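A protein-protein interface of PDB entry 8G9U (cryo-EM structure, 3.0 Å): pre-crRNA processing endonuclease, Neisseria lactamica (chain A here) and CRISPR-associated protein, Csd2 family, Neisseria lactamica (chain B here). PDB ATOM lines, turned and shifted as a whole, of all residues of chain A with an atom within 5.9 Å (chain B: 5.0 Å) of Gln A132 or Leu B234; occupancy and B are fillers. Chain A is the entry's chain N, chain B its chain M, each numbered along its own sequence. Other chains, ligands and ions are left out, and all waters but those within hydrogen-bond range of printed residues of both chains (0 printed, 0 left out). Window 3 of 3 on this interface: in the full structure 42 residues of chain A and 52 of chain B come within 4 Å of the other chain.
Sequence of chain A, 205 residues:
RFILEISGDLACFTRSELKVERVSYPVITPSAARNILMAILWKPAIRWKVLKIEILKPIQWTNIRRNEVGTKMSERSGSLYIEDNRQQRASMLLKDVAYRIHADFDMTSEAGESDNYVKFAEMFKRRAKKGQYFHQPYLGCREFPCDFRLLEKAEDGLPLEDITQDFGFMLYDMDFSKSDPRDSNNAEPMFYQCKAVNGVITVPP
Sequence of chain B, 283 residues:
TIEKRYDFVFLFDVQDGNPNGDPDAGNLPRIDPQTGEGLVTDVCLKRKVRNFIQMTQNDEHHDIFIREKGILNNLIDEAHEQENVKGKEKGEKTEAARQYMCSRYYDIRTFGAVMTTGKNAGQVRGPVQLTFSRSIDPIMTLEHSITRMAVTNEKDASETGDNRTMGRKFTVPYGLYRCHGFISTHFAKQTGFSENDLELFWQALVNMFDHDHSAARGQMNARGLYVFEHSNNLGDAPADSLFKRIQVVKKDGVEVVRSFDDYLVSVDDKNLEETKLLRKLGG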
ATOM      1  N   ALA A  39      19.737   1.159  12.257  1.00  0.00           N
ATOM      2  CA  ALA A  39      19.989   2.394  12.984  1.00  0.00           C
ATOM      3  C   ALA A  39      20.917   3.305  12.198  1.00  0.00           C
ATOM      4  O   ALA A  39      20.719   4.521  12.163  1.00  0.00           O
ATOM      5  CB  ALA A  39      20.572   2.085  14.358  1.00  0.00           C
ATOM      6  N   ILE A  40      21.937   2.740  11.560  1.00  0.00           N
ATOM      7  CA  ILE A  40      22.826   3.552  10.744  1.00  0.00           C
ATOM      8  C   ILE A  40      22.124   4.013   9.478  1.00  0.00           C
ATOM      9  O   ILE A  40      22.234   5.175   9.078  1.00  0.00           O
ATOM     10  CB  ILE A  40      24.115   2.782  10.435  1.00  0.00           C
ATOM     11  CG1 ILE A  40      24.956   2.700  11.696  1.00  0.00           C
ATOM     12  CG2 ILE A  40      24.889   3.473   9.359  1.00  0.00           C
ATOM     13  CD1 ILE A  40      26.292   2.144  11.465  1.00  0.00           C
ATOM     14  N   MET A 123      24.855   5.178   0.428  1.00  0.00           N
ATOM     15  CA  MET A 123      24.312   5.970   1.521  1.00  0.00           C
ATOM     16  C   MET A 123      24.737   5.385   2.857  1.00  0.00           C
ATOM     17  O   MET A 123      25.281   6.088   3.712  1.00  0.00           O
ATOM     18  CB  MET A 123      22.789   6.019   1.393  1.00  0.00           C
ATOM     19  CG  MET A 123      22.075   6.904   2.381  1.00  0.00           C
ATOM     20  SD  MET A 123      20.295   6.868   2.099  1.00  0.00           S
ATOM     21  CE  MET A 123      20.171   7.800   0.577  1.00  0.00           C
ATOM     22  N   ARG A 126      28.693   5.716   3.266  1.00  0.00           N
ATOM     23  CA  ARG A 126      29.037   7.041   3.760  1.00  0.00           C
ATOM     24  C   ARG A 126      28.601   7.221   5.200  1.00  0.00           C
ATOM     25  O   ARG A 126      29.335   7.807   5.998  1.00  0.00           O
ATOM     26  CB  ARG A 126      28.387   8.113   2.893  1.00  0.00           C
ATOM     27  CG  ARG A 126      28.935   8.211   1.487  1.00  0.00           C
ATOM     28  CD  ARG A 126      28.263   9.350   0.756  1.00  0.00           C
ATOM     29  NE  ARG A 126      26.862   9.049   0.495  1.00  0.00           N
ATOM     30  CZ  ARG A 126      25.846   9.691   1.059  1.00  0.00           C
ATOM     31  NH1 ARG A 126      26.079  10.660   1.930  1.00  0.00           N
ATOM     32  NH2 ARG A 126      24.599   9.356   0.762  1.00  0.00           N
ATOM     33  N   ARG A 127      27.414   6.729   5.551  1.00  0.00           N
ATOM     34  CA  ARG A 127      26.942   6.864   6.918  1.00  0.00           C
ATOM     35  C   ARG A 127      27.882   6.169   7.886  1.00  0.00           C
ATOM     36  O   ARG A 127      28.226   6.713   8.937  1.00  0.00           O
ATOM     37  CB  ARG A 127      25.532   6.295   7.036  1.00  0.00           C
ATOM     38  CG  ARG A 127      24.454   7.324   6.817  1.00  0.00           C
ATOM     39  CD  ARG A 127      23.170   6.679   6.402  1.00  0.00           C
ATOM     40  NE  ARG A 127      22.184   7.667   5.999  1.00  0.00           N
ATOM     41  CZ  ARG A 127      20.976   7.764   6.532  1.00  0.00           C
ATOM     42  NH1 ARG A 127      20.133   8.692   6.110  1.00  0.00           N
ATOM     43  NH2 ARG A 127      20.612   6.932   7.494  1.00  0.00           N
ATOM     44  N   ALA A 128      28.322   4.968   7.535  1.00  0.00           N
ATOM     45  CA  ALA A 128      29.105   4.175   8.468  1.00  0.00           C
ATOM     46  C   ALA A 128      30.540   4.677   8.562  1.00  0.00           C
ATOM     47  O   ALA A 128      31.080   4.818   9.665  1.00  0.00           O
ATOM     48  CB  ALA A 128      29.055   2.708   8.062  1.00  0.00           C
ATOM     49  N   LYS A 129      31.186   4.954   7.425  1.00  0.00           N
ATOM     50  CA  LYS A 129      32.537   5.507   7.501  1.00  0.00           C
ATOM     51  C   LYS A 129      32.531   6.878   8.156  1.00  0.00           C
ATOM     52  O   LYS A 129      33.325   7.146   9.063  1.00  0.00           O
ATOM     53  CB  LYS A 129      33.192   5.580   6.124  1.00  0.00           C
ATOM     54  CG  LYS A 129      33.485   4.249   5.477  1.00  0.00           C
ATOM     55  CD  LYS A 129      34.151   4.464   4.131  1.00  0.00           C
ATOM     56  CE  LYS A 129      34.553   3.150   3.495  1.00  0.00           C
ATOM     57  NZ  LYS A 129      33.388   2.324   3.123  1.00  0.00           N
ATOM     58  N   LYS A 130      31.642   7.763   7.706  1.00  0.00           N
ATOM     59  CA  LYS A 130      31.507   9.059   8.354  1.00  0.00           C
ATOM     60  C   LYS A 130      31.106   8.900   9.811  1.00  0.00           C
ATOM     61  O   LYS A 130      31.493   9.713  10.654  1.00  0.00           O
ATOM     62  CB  LYS A 130      30.484   9.912   7.605  1.00  0.00           C
ATOM     63  CG  LYS A 130      30.227  11.261   8.230  1.00  0.00           C
ATOM     64  CD  LYS A 130      31.224  12.294   7.757  1.00  0.00           C
ATOM     65  CE  LYS A 130      30.694  13.064   6.569  1.00  0.00           C
ATOM     66  NZ  LYS A 130      31.480  14.307   6.342  1.00  0.00           N
ATOM     67  N   GLY A 131      30.367   7.844  10.131  1.00  0.00           N
ATOM     68  CA  GLY A 131      29.836   7.647  11.458  1.00  0.00           C
ATOM     69  C   GLY A 131      28.392   8.055  11.611  1.00  0.00           C
ATOM     70  O   GLY A 131      27.879   8.042  12.735  1.00  0.00           O
ATOM     71  N   GLN A 132      27.725   8.421  10.522  1.00  0.00           N
ATOM     72  CA  GLN A 132      26.352   8.875  10.615  1.00  0.00           C
ATOM     73  C   GLN A 132      25.439   7.727  11.005  1.00  0.00           C
ATOM     74  O   GLN A 132      25.781   6.551  10.878  1.00  0.00           O
ATOM     75  CB  GLN A 132      25.887   9.480   9.293  1.00  0.00           C
ATOM     76  CG  GLN A 132      26.882  10.417   8.661  1.00  0.00           C
ATOM     77  CD  GLN A 132      26.411  10.977   7.341  1.00  0.00           C
ATOM     78  OE1 GLN A 132      27.179  11.595   6.609  1.00  0.00           O
ATOM     79  NE2 GLN A 132      25.146  10.756   7.023  1.00  0.00           N
ATOM     80  N   TYR A 133      24.271   8.095  11.510  1.00  0.00           N
ATOM     81  CA  TYR A 133      23.221   7.150  11.839  1.00  0.00           C
ATOM     82  C   TYR A 133      21.924   7.879  12.130  1.00  0.00           C
ATOM     83  O   TYR A 133      21.909   9.055  12.491  1.00  0.00           O
ATOM     84  CB  TYR A 133      23.593   6.253  13.019  1.00  0.00           C
ATOM     85  CG  TYR A 133      23.984   6.963  14.286  1.00  0.00           C
ATOM     86  CD1 TYR A 133      23.046   7.582  15.074  1.00  0.00           C
ATOM     87  CD2 TYR A 133      25.311   7.137  14.611  1.00  0.00           C
ATOM     88  CE1 TYR A 133      23.401   8.251  16.212  1.00  0.00           C
ATOM     89  CE2 TYR A 133      25.679   7.779  15.759  1.00  0.00           C
ATOM     90  CZ  TYR A 133      24.719   8.350  16.552  1.00  0.00           C
ATOM     91  OH  TYR A 133      25.076   9.031  17.691  1.00  0.00           O
ATOM     92  N   PHE A 134      20.833   7.146  11.959  1.00  0.00           N
ATOM     93  CA  PHE A 134      19.510   7.565  12.383  1.00  0.00           C
ATOM     94  C   PHE A 134      19.318   7.387  13.879  1.00  0.00           C
ATOM     95  O   PHE A 134      18.419   7.989  14.466  1.00  0.00           O
ATOM     96  CB  PHE A 134      18.493   6.733  11.613  1.00  0.00           C
ATOM     97  CG  PHE A 134      17.071   7.052  11.903  1.00  0.00           C
ATOM     98  CD1 PHE A 134      16.406   6.427  12.933  1.00  0.00           C
ATOM     99  CD2 PHE A 134      16.370   7.916  11.092  1.00  0.00           C
ATOM    100  CE1 PHE A 134      15.090   6.701  13.183  1.00  0.00           C
ATOM    101  CE2 PHE A 134      15.049   8.182  11.332  1.00  0.00           C
ATOM    102  CZ  PHE A 134      14.411   7.578  12.383  1.00  0.00           C
ATOM    103  N   PHE A 148      30.711   1.603  16.349  1.00  0.00           N
ATOM    104  CA  PHE A 148      30.854   0.819  15.131  1.00  0.00           C
ATOM    105  C   PHE A 148      32.003   1.336  14.277  1.00  0.00           C
ATOM    106  O   PHE A 148      32.794   2.192  14.681  1.00  0.00           O
ATOM    107  CB  PHE A 148      29.550   0.815  14.343  1.00  0.00           C
ATOM    108  CG  PHE A 148      29.093   2.170  13.915  1.00  0.00           C
ATOM    109  CD1 PHE A 148      28.257   2.916  14.721  1.00  0.00           C
ATOM    110  CD2 PHE A 148      29.480   2.693  12.700  1.00  0.00           C
ATOM    111  CE1 PHE A 148      27.831   4.157  14.332  1.00  0.00           C
ATOM    112  CE2 PHE A 148      29.059   3.936  12.304  1.00  0.00           C
ATOM    113  CZ  PHE A 148      28.230   4.668  13.119  1.00  0.00           C
ATOM    114  N   ARG B   5      22.126  16.285  15.365  1.00  0.00           N
ATOM    115  CA  ARG B   5      22.434  15.089  16.131  1.00  0.00           C
ATOM    116  C   ARG B   5      23.399  15.458  17.242  1.00  0.00           C
ATOM    117  O   ARG B   5      24.460  16.028  16.985  1.00  0.00           O
ATOM    118  CB  ARG B   5      23.034  14.006  15.245  1.00  0.00           C
ATOM    119  CG  ARG B   5      22.966  12.628  15.848  1.00  0.00           C
ATOM    120  CD  ARG B   5      23.839  11.693  15.076  1.00  0.00           C
ATOM    121  NE  ARG B   5      25.160  11.560  15.670  1.00  0.00           N
ATOM    122  CZ  ARG B   5      26.143  10.863  15.122  1.00  0.00           C
ATOM    123  NH1 ARG B   5      27.316  10.769  15.725  1.00  0.00           N
ATOM    124  NH2 ARG B   5      25.950  10.251  13.967  1.00  0.00           N
ATOM    125  N   HIS B 186      16.653  12.431  14.707  1.00  0.00           N
ATOM    126  CA  HIS B 186      15.689  11.611  14.001  1.00  0.00           C
ATOM    127  C   HIS B 186      14.561  11.175  14.914  1.00  0.00           C
ATOM    128  O   HIS B 186      13.400  11.164  14.500  1.00  0.00           O
ATOM    129  CB  HIS B 186      16.401  10.428  13.376  1.00  0.00           C
ATOM    130  CG  HIS B 186      17.373  10.825  12.317  1.00  0.00           C
ATOM    131  ND1 HIS B 186      16.970  11.222  11.061  1.00  0.00           N
ATOM    132  CD2 HIS B 186      18.720  10.930  12.332  1.00  0.00           C
ATOM    133  CE1 HIS B 186      18.031  11.529  10.338  1.00  0.00           C
ATOM    134  NE2 HIS B 186      19.106  11.362  11.086  1.00  0.00           N
ATOM    135  N   ASN B 232      24.671  17.813  10.669  1.00  0.00           N
ATOM    136  CA  ASN B 232      23.755  16.890  10.026  1.00  0.00           C
ATOM    137  C   ASN B 232      22.718  16.387  11.012  1.00  0.00           C
ATOM    138  O   ASN B 232      22.958  16.317  12.218  1.00  0.00           O
ATOM    139  CB  ASN B 232      24.503  15.694   9.445  1.00  0.00           C
ATOM    140  CG  ASN B 232      25.455  16.084   8.354  1.00  0.00           C
ATOM    141  OD1 ASN B 232      26.666  15.947   8.497  1.00  0.00           O
ATOM    142  ND2 ASN B 232      24.913  16.574   7.246  1.00  0.00           N
ATOM    143  N   ASN B 233      21.551  16.036  10.479  1.00  0.00           N
ATOM    144  CA  ASN B 233      20.650  15.176  11.227  1.00  0.00           C
ATOM    145  C   ASN B 233      21.306  13.835  11.496  1.00  0.00           C
ATOM    146  O   ASN B 233      21.215  13.295  12.603  1.00  0.00           O
ATOM    147  CB  ASN B 233      19.349  14.975  10.459  1.00  0.00           C
ATOM    148  CG  ASN B 233      18.639  16.269  10.181  1.00  0.00           C
ATOM    149  OD1 ASN B 233      19.245  17.339  10.208  1.00  0.00           O
ATOM    150  ND2 ASN B 233      17.344  16.185   9.909  1.00  0.00           N
ATOM    151  N   LEU B 234      21.989  13.290  10.494  1.00  0.00           N
ATOM    152  CA  LEU B 234      22.542  11.953  10.605  1.00  0.00           C
ATOM    153  C   LEU B 234      23.774  11.915  11.489  1.00  0.00           C
ATOM    154  O   LEU B 234      24.042  10.892  12.121  1.00  0.00           O
ATOM    155  CB  LEU B 234      22.883  11.411   9.221  1.00  0.00           C
ATOM    156  CG  LEU B 234      21.719  10.823   8.437  1.00  0.00           C
ATOM    157  CD1 LEU B 234      21.171   9.654   9.223  1.00  0.00           C
ATOM    158  CD2 LEU B 234      20.633  11.835   8.105  1.00  0.00           C
ATOM    159  N   GLY B 235      24.543  12.992  11.538  1.00  0.00           N
ATOM    160  CA  GLY B 235      25.680  13.018  12.430  1.00  0.00           C
ATOM    161  C   GLY B 235      26.993  12.765  11.734  1.00  0.00           C
ATOM    162  O   GLY B 235      27.336  11.633  11.405  1.00  0.00           O
ATOM    163  N   ASP B 236      27.756  13.822  11.558  1.00  0.00           N
ATOM    164  CA  ASP B 236      28.939  13.859  10.715  1.00  0.00           C
ATOM    165  C   ASP B 236      30.193  13.281  11.367  1.00  0.00           C
ATOM    166  O   ASP B 236      31.300  13.660  10.974  1.00  0.00           O
ATOM    167  CB  ASP B 236      29.148  15.298  10.250  1.00  0.00           C
ATOM    168  CG  ASP B 236      29.389  16.251  11.395  1.00  0.00           C
ATOM    169  OD1 ASP B 236      29.361  15.815  12.563  1.00  0.00           O
ATOM    170  OD2 ASP B 236      29.528  17.459  11.127  1.00  0.00           O
ATOM    171  N   ALA B 237      30.060  12.385  12.339  1.00  0.00           N
ATOM    172  CA  ALA B 237      31.211  11.805  13.016  1.00  0.00           C
ATOM    173  C   ALA B 237      30.868  10.386  13.429  1.00  0.00           C
ATOM    174  O   ALA B 237      29.689  10.038  13.543  1.00  0.00           O
ATOM    175  CB  ALA B 237      31.594  12.619  14.253  1.00  0.00           C
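NH2 of Arg B5 is in hydrogen-bond range of O of Gly A131 (3.2 Å). The side-chain hydroxyl (OH) of Tyr A133 lies within hydrogen-bond range of the guanidinium group (NE) of Arg B5 (3.2 Å). The backbone carbonyl oxygen (O) of Leu B234 is in hydrogen-bond range of the backbone NH (N) of Tyr A133 (2.9 Å). The backbone NH (N) of Gln A132 lies close to the backbone carbonyl oxygen (O) of Gly B235 (3.4 Å). The backbone NH (N) of Ala B237 lies close to the backbone carbonyl oxygen (O) of Lys A130 (3.5 Å). The backbone carbonyl oxygen (O) of Gly A131 lies close to the backbone carbonyl oxygen (O) of Ala B237 (2.8 Å).
O of Asn B232 lies within hydrogen-bond range of N of Arg B5 (3.3 Å). The guanidinium group of Arg B5 lies within hydrogen-bond range of the backbone carbonyl oxygen of Leu B234, at 2.7 Å. NH2 of Arg B5 lies close to O of Gly B235, 3.2 Å away. NH1 of Arg B5 sits at hydrogen-bond distance from O of Ala B237. NE2 of His B186 lies within hydrogen-bond range of O of Asn B233 (3.2 Å). The backbone carbonyl oxygen (O) of Ala A39 sits at hydrogen-bond distance from the backbone NH (N) of Phe A134.
Among the printed residues, pairs that only touch across the chains: Gln A132 with Leu B234 (3.2 Å), Arg A127 with Leu B234 (3.3 Å), Phe A134 with His B186 (3.3 Å), Lys A130 with Asp B236 (3.5 Å), Gln A132 with Arg B5 (3.6 Å), Tyr A133 with His B186 (3.7 Å), Phe A134 with Leu B234 (3.7 Å), Gly A131 with Gly B235 (3.7 Å) and Gln A132 with Ala B237 (3.9 Å).
Of the printed residues of chain B, Gly A131 touches Arg B5, Gly B235 and Ala B237. Of the printed residues of chain B, Gln A132 touches Arg B5, Leu B234, Gly B235 and Ala B237. Of the printed residues of chain B, Phe A134 touches His B186 and Leu B234. Of the printed residues of chain A, Arg B5 touches Gly A131 (3.2 Å), Gln A132 (3.6 Å) and Tyr A133 (3.1 Å). Of the printed residues of chain A, Leu B234 touches Arg A127 (3.3 Å), Gln A132 (3.2 Å), Tyr A133 (2.8 Å) and Phe A134 (3.7 Å). Printed residues of chain A within 4 Å of Gly B235: Gly A131 (3.7 Å) and Gln A132 (3.0 Å). Of the printed residues of chain A, Ala B237 touches Lys A130 (2.9 Å), Gly A131 (2.8 Å) and Gln A132 (3.9 Å). The nearest residue of chain A that does not touch Leu B234 is Ile A40 (4.6 Å). The nearest printed residue of chain B that does not touch Lys A130 is Gly B235 (4.3 Å).
Hydrophobic or aromatic side chains of chain B that line the printed part of chain A: His B186 and Leu B234. Printed residues of chain A that touch a printed residue of chain B: Arg A127, Lys A130, Gly A131, Gln A132, Tyr A133 and Phe A134. Hydrophobic or aromatic side chains of chain A within 4 Å of the printed part of chain B: Tyr A133 and Phe A134.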
